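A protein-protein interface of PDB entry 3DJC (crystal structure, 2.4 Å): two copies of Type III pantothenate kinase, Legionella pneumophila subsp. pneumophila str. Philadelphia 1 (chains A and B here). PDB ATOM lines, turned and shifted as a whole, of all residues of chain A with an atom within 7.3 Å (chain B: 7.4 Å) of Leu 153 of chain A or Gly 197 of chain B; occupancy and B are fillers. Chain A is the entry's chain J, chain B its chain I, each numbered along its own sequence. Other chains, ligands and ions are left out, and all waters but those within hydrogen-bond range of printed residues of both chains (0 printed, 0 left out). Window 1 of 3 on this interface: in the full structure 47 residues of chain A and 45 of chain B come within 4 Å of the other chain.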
ATOM      1  N   ASP A 131      -4.567 -18.360 -19.292  1.00  0.00           N
ATOM      2  CA  ASP A 131      -4.437 -18.607 -20.725  1.00  0.00           C
ATOM      3  C   ASP A 131      -3.434 -19.735 -20.940  1.00  0.00           C
ATOM      4  O   ASP A 131      -2.226 -19.532 -20.835  1.00  0.00           O
ATOM      5  CB  ASP A 131      -4.034 -17.327 -21.478  1.00  0.00           C
ATOM      6  CG  ASP A 131      -3.993 -17.505 -23.006  1.00  0.00           C
ATOM      7  OD1 ASP A 131      -3.384 -16.645 -23.674  1.00  0.00           O
ATOM      8  OD2 ASP A 131      -4.556 -18.479 -23.552  1.00  0.00           O
ATOM      9  N   GLY A 133      -1.623 -21.266 -23.259  1.00  0.00           N
ATOM     10  CA  GLY A 133      -1.116 -21.112 -24.618  1.00  0.00           C
ATOM     11  C   GLY A 133       0.351 -21.472 -24.730  1.00  0.00           C
ATOM     12  O   GLY A 133       0.810 -22.450 -24.122  1.00  0.00           O
ATOM     13  N   THR A 134       1.069 -20.676 -25.527  1.00  0.00           N
ATOM     14  CA  THR A 134       2.530 -20.731 -25.656  1.00  0.00           C
ATOM     15  C   THR A 134       3.150 -20.556 -24.283  1.00  0.00           C
ATOM     16  O   THR A 134       4.026 -21.318 -23.872  1.00  0.00           O
ATOM     17  CB  THR A 134       3.043 -19.600 -26.569  1.00  0.00           C
ATOM     18  OG1 THR A 134       2.085 -19.348 -27.602  1.00  0.00           O
ATOM     19  CG2 THR A 134       4.372 -19.977 -27.199  1.00  0.00           C
ATOM     20  N   ALA A 135       2.677 -19.529 -23.588  1.00  0.00           N
ATOM     21  CA  ALA A 135       2.906 -19.375 -22.170  1.00  0.00           C
ATOM     22  C   ALA A 135       1.603 -19.684 -21.438  1.00  0.00           C
ATOM     23  O   ALA A 135       0.519 -19.289 -21.888  1.00  0.00           O
ATOM     24  CB  ALA A 135       3.350 -17.973 -21.870  1.00  0.00           C
ATOM     25  N   THR A 136       1.712 -20.420 -20.333  1.00  0.00           N
ATOM     26  CA  THR A 136       0.612 -20.554 -19.392  1.00  0.00           C
ATOM     27  C   THR A 136       0.671 -19.316 -18.501  1.00  0.00           C
ATOM     28  O   THR A 136       1.584 -19.164 -17.688  1.00  0.00           O
ATOM     29  CB  THR A 136       0.704 -21.858 -18.564  1.00  0.00           C
ATOM     30  OG1 THR A 136       0.737 -22.984 -19.450  1.00  0.00           O
ATOM     31  CG2 THR A 136      -0.493 -22.002 -17.625  1.00  0.00           C
ATOM     32  N   THR A 137      -0.288 -18.417 -18.689  1.00  0.00           N
ATOM     33  CA  THR A 137      -0.286 -17.134 -17.994  1.00  0.00           C
ATOM     34  C   THR A 137      -1.419 -17.041 -16.983  1.00  0.00           C
ATOM     35  O   THR A 137      -2.449 -17.712 -17.122  1.00  0.00           O
ATOM     36  CB  THR A 137      -0.372 -15.942 -18.970  1.00  0.00           C
ATOM     37  OG1 THR A 137      -1.561 -16.049 -19.758  1.00  0.00           O
ATOM     38  CG2 THR A 137       0.830 -15.910 -19.895  1.00  0.00           C
ATOM     39  N   PHE A 138      -1.200 -16.214 -15.962  1.00  0.00           N
ATOM     40  CA  PHE A 138      -2.162 -15.987 -14.898  1.00  0.00           C
ATOM     41  C   PHE A 138      -2.359 -14.479 -14.747  1.00  0.00           C
ATOM     42  O   PHE A 138      -1.389 -13.721 -14.790  1.00  0.00           O
ATOM     43  CB  PHE A 138      -1.652 -16.619 -13.598  1.00  0.00           C
ATOM     44  CG  PHE A 138      -1.644 -18.130 -13.615  1.00  0.00           C
ATOM     45  CD1 PHE A 138      -0.586 -18.838 -14.193  1.00  0.00           C
ATOM     46  CD2 PHE A 138      -2.687 -18.846 -13.038  1.00  0.00           C
ATOM     47  CE1 PHE A 138      -0.581 -20.232 -14.219  1.00  0.00           C
ATOM     48  CE2 PHE A 138      -2.683 -20.244 -13.049  1.00  0.00           C
ATOM     49  CZ  PHE A 138      -1.626 -20.933 -13.648  1.00  0.00           C
ATOM     50  N   ALA A 151       1.411 -13.764 -13.304  1.00  0.00           N
ATOM     51  CA  ALA A 151       2.476 -14.749 -13.446  1.00  0.00           C
ATOM     52  C   ALA A 151       2.542 -15.284 -14.874  1.00  0.00           C
ATOM     53  O   ALA A 151       1.526 -15.325 -15.572  1.00  0.00           O
ATOM     54  CB  ALA A 151       2.253 -15.892 -12.472  1.00  0.00           C
ATOM     55  N   ILE A 152       3.742 -15.679 -15.303  1.00  0.00           N
ATOM     56  CA  ILE A 152       3.953 -16.289 -16.619  1.00  0.00           C
ATOM     57  C   ILE A 152       4.799 -17.565 -16.499  1.00  0.00           C
ATOM     58  O   ILE A 152       5.966 -17.514 -16.110  1.00  0.00           O
ATOM     59  CB  ILE A 152       4.633 -15.322 -17.637  1.00  0.00           C
ATOM     60  CG1 ILE A 152       3.825 -14.034 -17.841  1.00  0.00           C
ATOM     61  CG2 ILE A 152       4.830 -16.011 -18.981  1.00  0.00           C
ATOM     62  CD1 ILE A 152       4.571 -12.951 -18.634  1.00  0.00           C
ATOM     63  N   LEU A 153       4.192 -18.699 -16.836  1.00  0.00           N
ATOM     64  CA  LEU A 153       4.877 -19.987 -16.916  1.00  0.00           C
ATOM     65  C   LEU A 153       5.084 -20.368 -18.382  1.00  0.00           C
ATOM     66  O   LEU A 153       4.364 -19.867 -19.243  1.00  0.00           O
ATOM     67  CB  LEU A 153       4.017 -21.062 -16.256  1.00  0.00           C
ATOM     68  CG  LEU A 153       4.188 -21.394 -14.782  1.00  0.00           C
ATOM     69  CD1 LEU A 153       2.904 -22.011 -14.311  1.00  0.00           C
ATOM     70  CD2 LEU A 153       5.358 -22.355 -14.580  1.00  0.00           C
ATOM     71  N   PRO A 154       6.071 -21.248 -18.679  1.00  0.00           N
ATOM     72  CA  PRO A 154       6.086 -21.809 -20.028  1.00  0.00           C
ATOM     73  C   PRO A 154       4.911 -22.759 -20.219  1.00  0.00           C
ATOM     74  O   PRO A 154       4.484 -23.413 -19.266  1.00  0.00           O
ATOM     75  CB  PRO A 154       7.412 -22.574 -20.083  1.00  0.00           C
ATOM     76  CG  PRO A 154       7.735 -22.885 -18.673  1.00  0.00           C
ATOM     77  CD  PRO A 154       7.199 -21.745 -17.866  1.00  0.00           C
ATOM     78  N   GLY A 155       4.383 -22.815 -21.437  1.00  0.00           N
ATOM     79  CA  GLY A 155       3.205 -23.622 -21.727  1.00  0.00           C
ATOM     80  C   GLY A 155       3.516 -25.100 -21.800  1.00  0.00           C
ATOM     81  O   GLY A 155       4.671 -25.503 -21.676  1.00  0.00           O
ATOM     82  N   LEU A 156       2.474 -25.899 -22.021  1.00  0.00           N
ATOM     83  CA  LEU A 156       2.585 -27.357 -22.045  1.00  0.00           C
ATOM     84  C   LEU A 156       3.434 -27.871 -23.207  1.00  0.00           C
ATOM     85  O   LEU A 156       4.128 -28.877 -23.066  1.00  0.00           O
ATOM     86  CB  LEU A 156       1.195 -28.013 -22.050  1.00  0.00           C
ATOM     87  CG  LEU A 156       0.444 -28.095 -20.712  1.00  0.00           C
ATOM     88  CD1 LEU A 156      -0.333 -26.815 -20.378  1.00  0.00           C
ATOM     89  CD2 LEU A 156      -0.494 -29.274 -20.715  1.00  0.00           C
ATOM     90  N   LEU A 158       5.938 -25.962 -24.916  1.00  0.00           N
ATOM     91  CA  LEU A 158       7.322 -25.502 -24.716  1.00  0.00           C
ATOM     92  C   LEU A 158       8.048 -26.229 -23.587  1.00  0.00           C
ATOM     93  O   LEU A 158       9.263 -26.391 -23.644  1.00  0.00           O
ATOM     94  CB  LEU A 158       7.386 -23.989 -24.454  1.00  0.00           C
ATOM     95  CG  LEU A 158       6.760 -22.937 -25.378  1.00  0.00           C
ATOM     96  CD1 LEU A 158       7.260 -21.565 -24.956  1.00  0.00           C
ATOM     97  CD2 LEU A 158       7.062 -23.174 -26.852  1.00  0.00           C
ATOM     98  N   SER A 159       7.301 -26.645 -22.565  1.00  0.00           N
ATOM     99  CA  SER A 159       7.854 -27.378 -21.423  1.00  0.00           C
ATOM    100  C   SER A 159       8.329 -28.773 -21.826  1.00  0.00           C
ATOM    101  O   SER A 159       9.466 -29.163 -21.521  1.00  0.00           O
ATOM    102  CB  SER A 159       6.817 -27.487 -20.305  1.00  0.00           C
ATOM    103  OG  SER A 159       6.415 -26.204 -19.861  1.00  0.00           O
ATOM    104  N   GLY A 197       2.239 -31.432 -13.227  1.00  0.00           N
ATOM    105  CA  GLY A 197       3.062 -30.271 -12.919  1.00  0.00           C
ATOM    106  C   GLY A 197       2.333 -28.975 -13.157  1.00  0.00           C
ATOM    107  O   GLY A 197       2.373 -28.089 -12.309  1.00  0.00           O
ATOM    108  N   VAL A 198       1.673 -28.864 -14.311  1.00  0.00           N
ATOM    109  CA  VAL A 198       0.845 -27.695 -14.640  1.00  0.00           C
ATOM    110  C   VAL A 198      -0.424 -27.690 -13.778  1.00  0.00           C
ATOM    111  O   VAL A 198      -0.899 -26.629 -13.391  1.00  0.00           O
ATOM    112  CB  VAL A 198       0.514 -27.603 -16.166  1.00  0.00           C
ATOM    113  CG1 VAL A 198      -0.357 -26.388 -16.480  1.00  0.00           C
ATOM    114  CG2 VAL A 198       1.777 -27.498 -16.976  1.00  0.00           C
ATOM    115  N   GLY A 200      -0.611 -28.757 -10.651  1.00  0.00           N
ATOM    116  CA  GLY A 200      -0.159 -28.213  -9.377  1.00  0.00           C
ATOM    117  C   GLY A 200       0.286 -26.766  -9.466  1.00  0.00           C
ATOM    118  O   GLY A 200       0.127 -26.009  -8.504  1.00  0.00           O
ATOM    119  N   ALA A 201       0.853 -26.390 -10.614  1.00  0.00           N
ATOM    120  CA  ALA A 201       1.266 -25.006 -10.878  1.00  0.00           C
ATOM    121  C   ALA A 201       0.066 -24.073 -10.834  1.00  0.00           C
ATOM    122  O   ALA A 201       0.130 -23.001 -10.238  1.00  0.00           O
ATOM    123  CB  ALA A 201       1.957 -24.901 -12.218  1.00  0.00           C
ATOM    124  N   CYS A 202      -1.022 -24.506 -11.463  1.00  0.00           N
ATOM    125  CA  CYS A 202      -2.301 -23.813 -11.395  1.00  0.00           C
ATOM    126  C   CYS A 202      -2.809 -23.712  -9.963  1.00  0.00           C
ATOM    127  O   CYS A 202      -3.041 -22.613  -9.481  1.00  0.00           O
ATOM    128  CB  CYS A 202      -3.329 -24.513 -12.274  1.00  0.00           C
ATOM    129  SG  CYS A 202      -2.969 -24.383 -14.023  1.00  0.00           S
ATOM    130  N   GLU A 204      -1.306 -23.868  -7.190  1.00  0.00           N
ATOM    131  CA  GLU A 204      -0.474 -22.975  -6.396  1.00  0.00           C
ATOM    132  C   GLU A 204      -0.658 -21.515  -6.809  1.00  0.00           C
ATOM    133  O   GLU A 204      -0.846 -20.657  -5.954  1.00  0.00           O
ATOM    134  CB  GLU A 204       0.999 -23.373  -6.498  1.00  0.00           C
ATOM    135  CG  GLU A 204       1.905 -22.734  -5.454  1.00  0.00           C
ATOM    136  CD  GLU A 204       1.806 -23.372  -4.081  1.00  0.00           C
ATOM    137  OE1 GLU A 204       2.154 -22.691  -3.095  1.00  0.00           O
ATOM    138  OE2 GLU A 204       1.390 -24.545  -3.975  1.00  0.00           O
ATOM    139  N   LEU A 205      -0.616 -21.236  -8.111  1.00  0.00           N
ATOM    140  CA  LEU A 205      -0.758 -19.858  -8.594  1.00  0.00           C
ATOM    141  C   LEU A 205      -2.174 -19.302  -8.488  1.00  0.00           C
ATOM    142  O   LEU A 205      -2.355 -18.087  -8.481  1.00  0.00           O
ATOM    143  CB  LEU A 205      -0.195 -19.687 -10.009  1.00  0.00           C
ATOM    144  CG  LEU A 205       1.330 -19.574 -10.080  1.00  0.00           C
ATOM    145  CD1 LEU A 205       1.830 -19.749 -11.494  1.00  0.00           C
ATOM    146  CD2 LEU A 205       1.800 -18.245  -9.529  1.00  0.00           C
ATOM    147  N   LEU B 153      10.140 -33.116 -15.253  1.00  0.00           N
ATOM    148  CA  LEU B 153       9.712 -31.747 -15.565  1.00  0.00           C
ATOM    149  C   LEU B 153      10.871 -30.947 -16.161  1.00  0.00           C
ATOM    150  O   LEU B 153      12.030 -31.289 -15.919  1.00  0.00           O
ATOM    151  CB  LEU B 153       9.250 -31.044 -14.283  1.00  0.00           C
ATOM    152  CG  LEU B 153       7.787 -31.035 -13.848  1.00  0.00           C
ATOM    153  CD1 LEU B 153       7.700 -30.528 -12.421  1.00  0.00           C
ATOM    154  CD2 LEU B 153       6.943 -30.167 -14.763  1.00  0.00           C
ATOM    155  N   SER B 159      12.714 -23.963 -17.974  1.00  0.00           N
ATOM    156  CA  SER B 159      11.450 -23.237 -17.807  1.00  0.00           C
ATOM    157  C   SER B 159      11.571 -21.717 -17.960  1.00  0.00           C
ATOM    158  O   SER B 159      10.568 -21.032 -18.199  1.00  0.00           O
ATOM    159  CB  SER B 159      10.830 -23.562 -16.443  1.00  0.00           C
ATOM    160  OG  SER B 159      10.811 -24.961 -16.215  1.00  0.00           O
ATOM    161  N   LEU B 163      10.757 -19.793 -22.313  1.00  0.00           N
ATOM    162  CA  LEU B 163       9.919 -18.607 -22.431  1.00  0.00           C
ATOM    163  C   LEU B 163      10.513 -17.480 -23.279  1.00  0.00           C
ATOM    164  O   LEU B 163       9.766 -16.694 -23.844  1.00  0.00           O
ATOM    165  CB  LEU B 163       9.524 -18.083 -21.045  1.00  0.00           C
ATOM    166  CG  LEU B 163       8.185 -18.602 -20.515  1.00  0.00           C
ATOM    167  CD1 LEU B 163       8.031 -18.332 -19.036  1.00  0.00           C
ATOM    168  CD2 LEU B 163       7.038 -17.976 -21.287  1.00  0.00           C
ATOM    169  N   VAL B 181       3.368 -13.303  -6.221  1.00  0.00           N
ATOM    170  CA  VAL B 181       2.882 -14.024  -7.403  1.00  0.00           C
ATOM    171  C   VAL B 181       2.242 -13.047  -8.391  1.00  0.00           C
ATOM    172  O   VAL B 181       2.009 -13.387  -9.555  1.00  0.00           O
ATOM    173  CB  VAL B 181       1.876 -15.139  -7.052  1.00  0.00           C
ATOM    174  CG1 VAL B 181       2.582 -16.287  -6.377  1.00  0.00           C
ATOM    175  CG2 VAL B 181       0.753 -14.603  -6.178  1.00  0.00           C
ATOM    176  N   SER B 189       6.934 -11.116 -13.587  1.00  0.00           N
ATOM    177  CA  SER B 189       5.880 -12.078 -13.933  1.00  0.00           C
ATOM    178  C   SER B 189       6.410 -13.483 -14.214  1.00  0.00           C
ATOM    179  O   SER B 189       5.824 -14.471 -13.761  1.00  0.00           O
ATOM    180  CB  SER B 189       5.061 -11.587 -15.135  1.00  0.00           C
ATOM    181  OG  SER B 189       4.261 -10.467 -14.802  1.00  0.00           O
ATOM    182  N   ILE B 190       7.510 -13.568 -14.962  1.00  0.00           N
ATOM    183  CA  ILE B 190       8.145 -14.862 -15.237  1.00  0.00           C
ATOM    184  C   ILE B 190       8.757 -15.444 -13.956  1.00  0.00           C
ATOM    185  O   ILE B 190       8.553 -16.615 -13.674  1.00  0.00           O
ATOM    186  CB  ILE B 190       9.120 -14.834 -16.482  1.00  0.00           C
ATOM    187  CG1 ILE B 190       9.951 -16.124 -16.586  1.00  0.00           C
ATOM    188  CG2 ILE B 190      10.021 -13.616 -16.462  1.00  0.00           C
ATOM    189  CD1 ILE B 190      10.856 -16.201 -17.807  1.00  0.00           C
ATOM    190  N   GLN B 191       9.445 -14.617 -13.165  1.00  0.00           N
ATOM    191  CA  GLN B 191       9.991 -15.038 -11.860  1.00  0.00           C
ATOM    192  C   GLN B 191       8.947 -15.562 -10.866  1.00  0.00           C
ATOM    193  O   GLN B 191       9.179 -16.565 -10.198  1.00  0.00           O
ATOM    194  CB  GLN B 191      10.777 -13.904 -11.209  1.00  0.00           C
ATOM    195  CG  GLN B 191      12.143 -13.675 -11.819  1.00  0.00           C
ATOM    196  CD  GLN B 191      12.801 -12.412 -11.313  1.00  0.00           C
ATOM    197  OE1 GLN B 191      12.132 -11.504 -10.820  1.00  0.00           O
ATOM    198  NE2 GLN B 191      14.125 -12.353 -11.414  1.00  0.00           N
ATOM    199  N   SER B 192       7.810 -14.880 -10.780  1.00  0.00           N
ATOM    200  CA  SER B 192       6.683 -15.301  -9.948  1.00  0.00           C
ATOM    201  C   SER B 192       6.024 -16.593 -10.445  1.00  0.00           C
ATOM    202  O   SER B 192       5.452 -17.344  -9.654  1.00  0.00           O
ATOM    203  CB  SER B 192       5.636 -14.186  -9.879  1.00  0.00           C
ATOM    204  OG  SER B 192       6.216 -12.975  -9.424  1.00  0.00           O
ATOM    205  N   GLY B 193       6.097 -16.830 -11.753  1.00  0.00           N
ATOM    206  CA  GLY B 193       5.568 -18.043 -12.370  1.00  0.00           C
ATOM    207  C   GLY B 193       6.552 -19.192 -12.315  1.00  0.00           C
ATOM    208  O   GLY B 193       6.170 -20.326 -12.057  1.00  0.00           O
ATOM    209  N   VAL B 194       7.825 -18.885 -12.544  1.00  0.00           N
ATOM    210  CA  VAL B 194       8.912 -19.876 -12.579  1.00  0.00           C
ATOM    211  C   VAL B 194       9.381 -20.305 -11.172  1.00  0.00           C
ATOM    212  O   VAL B 194      10.016 -21.347 -11.017  1.00  0.00           O
ATOM    213  CB  VAL B 194      10.071 -19.375 -13.514  1.00  0.00           C
ATOM    214  CG1 VAL B 194      11.420 -20.023 -13.218  1.00  0.00           C
ATOM    215  CG2 VAL B 194       9.678 -19.564 -14.977  1.00  0.00           C
ATOM    216  N   TYR B 195       9.037 -19.525 -10.148  1.00  0.00           N
ATOM    217  CA  TYR B 195       9.272 -19.948  -8.763  1.00  0.00           C
ATOM    218  C   TYR B 195       8.054 -20.635  -8.130  1.00  0.00           C
ATOM    219  O   TYR B 195       8.203 -21.653  -7.448  1.00  0.00           O
ATOM    220  CB  TYR B 195       9.761 -18.784  -7.877  1.00  0.00           C
ATOM    221  CG  TYR B 195      10.142 -19.217  -6.474  1.00  0.00           C
ATOM    222  CD1 TYR B 195      11.370 -19.828  -6.220  1.00  0.00           C
ATOM    223  CD2 TYR B 195       9.269 -19.033  -5.406  1.00  0.00           C
ATOM    224  CE1 TYR B 195      11.717 -20.241  -4.932  1.00  0.00           C
ATOM    225  CE2 TYR B 195       9.599 -19.443  -4.123  1.00  0.00           C
ATOM    226  CZ  TYR B 195      10.825 -20.046  -3.894  1.00  0.00           C
ATOM    227  OH  TYR B 195      11.158 -20.450  -2.625  1.00  0.00           O
ATOM    228  N   TYR B 196       6.863 -20.075  -8.341  1.00  0.00           N
ATOM    229  CA  TYR B 196       5.640 -20.613  -7.724  1.00  0.00           C
ATOM    230  C   TYR B 196       4.893 -21.624  -8.593  1.00  0.00           C
ATOM    231  O   TYR B 196       4.003 -22.327  -8.106  1.00  0.00           O
ATOM    232  CB  TYR B 196       4.713 -19.484  -7.245  1.00  0.00           C
ATOM    233  CG  TYR B 196       5.309 -18.696  -6.099  1.00  0.00           C
ATOM    234  CD1 TYR B 196       5.194 -19.151  -4.782  1.00  0.00           C
ATOM    235  CD2 TYR B 196       6.016 -17.513  -6.330  1.00  0.00           C
ATOM    236  CE1 TYR B 196       5.759 -18.443  -3.724  1.00  0.00           C
ATOM    237  CE2 TYR B 196       6.578 -16.797  -5.278  1.00  0.00           C
ATOM    238  CZ  TYR B 196       6.452 -17.271  -3.981  1.00  0.00           C
ATOM    239  OH  TYR B 196       7.015 -16.570  -2.943  1.00  0.00           O
ATOM    240  N   GLY B 197       5.256 -21.697  -9.871  1.00  0.00           N
ATOM    241  CA  GLY B 197       4.745 -22.743 -10.746  1.00  0.00           C
ATOM    242  C   GLY B 197       5.419 -24.060 -10.429  1.00  0.00           C
ATOM    243  O   GLY B 197       4.766 -25.101 -10.406  1.00  0.00           O
ATOM    244  N   VAL B 198       6.726 -24.002 -10.167  1.00  0.00           N
ATOM    245  CA  VAL B 198       7.518 -25.184  -9.816  1.00  0.00           C
ATOM    246  C   VAL B 198       7.244 -25.636  -8.378  1.00  0.00           C
ATOM    247  O   VAL B 198       7.154 -26.838  -8.109  1.00  0.00           O
ATOM    248  CB  VAL B 198       9.040 -24.959 -10.050  1.00  0.00           C
ATOM    249  CG1 VAL B 198       9.827 -26.207  -9.697  1.00  0.00           C
ATOM    250  CG2 VAL B 198       9.307 -24.583 -11.505  1.00  0.00           C
ATOM    251  N   LEU B 199       7.094 -24.672  -7.470  1.00  0.00           N
ATOM    252  CA  LEU B 199       6.750 -24.956  -6.071  1.00  0.00           C
ATOM    253  C   LEU B 199       5.475 -25.784  -5.945  1.00  0.00           C
ATOM    254  O   LEU B 199       5.433 -26.732  -5.167  1.00  0.00           O
ATOM    255  CB  LEU B 199       6.647 -23.661  -5.249  1.00  0.00           C
ATOM    256  CG  LEU B 199       6.313 -23.716  -3.748  1.00  0.00           C
ATOM    257  CD1 LEU B 199       7.298 -24.566  -2.943  1.00  0.00           C
ATOM    258  CD2 LEU B 199       6.239 -22.309  -3.181  1.00  0.00           C
ATOM    259  N   GLY B 200       4.454 -25.430  -6.722  1.00  0.00           N
ATOM    260  CA  GLY B 200       3.195 -26.170  -6.729  1.00  0.00           C
ATOM    261  C   GLY B 200       3.244 -27.452  -7.536  1.00  0.00           C
ATOM    262  O   GLY B 200       2.514 -28.405  -7.239  1.00  0.00           O
ATOM    263  N   ALA B 201       4.094 -27.460  -8.563  1.00  0.00           N
ATOM    264  CA  ALA B 201       4.346 -28.644  -9.385  1.00  0.00           C
ATOM    265  C   ALA B 201       5.010 -29.734  -8.568  1.00  0.00           C
ATOM    266  O   ALA B 201       4.685 -30.912  -8.722  1.00  0.00           O
ATOM    267  CB  ALA B 201       5.222 -28.291 -10.575  1.00  0.00           C
ATOM    268  N   CYS B 202       5.950 -29.325  -7.715  1.00  0.00           N
ATOM    269  CA  CYS B 202       6.648 -30.225  -6.805  1.00  0.00           C
ATOM    270  C   CYS B 202       5.688 -30.764  -5.759  1.00  0.00           C
ATOM    271  O   CYS B 202       5.687 -31.957  -5.485  1.00  0.00           O
ATOM    272  CB  CYS B 202       7.815 -29.508  -6.125  1.00  0.00           C
ATOM    273  SG  CYS B 202       9.252 -29.184  -7.175  1.00  0.00           S
ATOM    274  N   LYS B 203       4.864 -29.872  -5.204  1.00  0.00           N
ATOM    275  CA  LYS B 203       3.845 -30.205  -4.205  1.00  0.00           C
ATOM    276  C   LYS B 203       2.812 -31.218  -4.702  1.00  0.00           C
ATOM    277  O   LYS B 203       2.366 -32.072  -3.944  1.00  0.00           O
ATOM    278  CB  LYS B 203       3.123 -28.936  -3.747  1.00  0.00           C
ATOM    279  CG  LYS B 203       3.854 -28.099  -2.711  1.00  0.00           C
ATOM    280  CD  LYS B 203       2.943 -26.990  -2.206  1.00  0.00           C
ATOM    281  CE  LYS B 203       3.713 -25.876  -1.524  1.00  0.00           C
ATOM    282  NZ  LYS B 203       2.817 -24.734  -1.191  1.00  0.00           N
ATOM    283  N   PHE B 231      14.131 -23.961  -2.575  1.00  0.00           N
ATOM    284  CA  PHE B 231      12.889 -24.476  -2.004  1.00  0.00           C
ATOM    285  C   PHE B 231      13.129 -25.025  -0.602  1.00  0.00           C
ATOM    286  O   PHE B 231      12.343 -25.837  -0.101  1.00  0.00           O
ATOM    287  CB  PHE B 231      12.310 -25.581  -2.901  1.00  0.00           C
ATOM    288  CG  PHE B 231      11.917 -25.113  -4.276  1.00  0.00           C
ATOM    289  CD1 PHE B 231      10.653 -24.583  -4.511  1.00  0.00           C
ATOM    290  CD2 PHE B 231      12.809 -25.212  -5.340  1.00  0.00           C
ATOM    291  CE1 PHE B 231      10.292 -24.147  -5.777  1.00  0.00           C
ATOM    292  CE2 PHE B 231      12.453 -24.778  -6.611  1.00  0.00           C
ATOM    293  CZ  PHE B 231      11.191 -24.244  -6.830  1.00  0.00           C
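CA of Ala 151 of chain A touches O of Ser 189 of chain B, at 3.4 Å. Ala 151 of chain A touches Gly 193 of chain B. Leu 163 of chain B touches Ile 152 of chain A. Gly 193 of chain B touches Ile 152 of chain A (CA to O, 3.8 Å). Leu 153 of chain A touches Gly 197 of chain B (CD2 to CA, 3.9 Å). Gly 197 of chain A touches Ala 201 of chain B (O to CB, 3.3 Å). Gly 197 of chain B touches Ala 201 of chain A. N of Ala 201 of chain B touches N of Ala 201 of chain A, at 3.98 Å. Leu 205 of chain A touches Val 181 of chain B. CD2 of Leu 205 of chain A touches CB of Tyr 196 of chain B, 3.9 Å away.
O of Pro 154 of chain A sits at hydrogen-bond distance from OG of Ser 159 of chain A. The backbone carbonyl oxygen (O) of Ala 151 of chain A is in hydrogen-bond range of the backbone NH (N) of Phe 138 of chain A, at 2.9 Å. The backbone carbonyl oxygen of Thr 136 of chain A sits at hydrogen-bond distance from the backbone NH of Leu 153 of chain A (2.8 Å).
Of chain B, only Leu 163 (3.6 Å), Gly 193 (3.3 Å) and Gly 197 (3.9 Å) come within 4 Å of Leu 153 of chain A. Printed residues of chain B within 4 Å of Ala 151 of chain A: Val 181, Ser 189 and Gly 193. Printed residues of chain B within 4 Å of Ala 135 of chain A: Leu 163. Cys 202 of chain A touches none of the printed residues of chain B. The nearest residue of chain B that does not touch Leu 153 of chain A is Val 194 of chain B (4.7 Å). The nearest printed residue of chain A that does not touch Gly 197 of chain B is Leu 205 of chain A (4.2 Å).
Leu 153 of chain A touches Gly 197 of chain B, but with the chains exchanged Gly 197 of chain A does not touch Leu 153 of chain B (4.3 Å). Gly 197 of chain A touches Ala 201 of chain B, and with the chains exchanged Ala 201 of chain A touches Gly 197 of chain B. Gly 200 of chain A touches its own counterpart, Gly 200 of chain B. Ala 201 of chain B touches its own counterpart, Ala 201 of chain A. Of the 24 pairs that touch across the chains among the printed residues, 4 have their exchanged pair printed and touching as well.
Of the 20 printed residues of chain B, 12 touch a printed residue of chain A. Among the printed residues, 24 pairs touch across the chains.
The side-chain amino group of Lys 203 of chain B is in salt-bridge range of the side-chain carboxylate of Glu 204 of chain A (2.9 Å). The backbone carbonyl oxygen (O) of Ser 189 of chain B lies within hydrogen-bond range of the backbone NH (N) of Ile 152 of chain A, at 2.9 Å.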
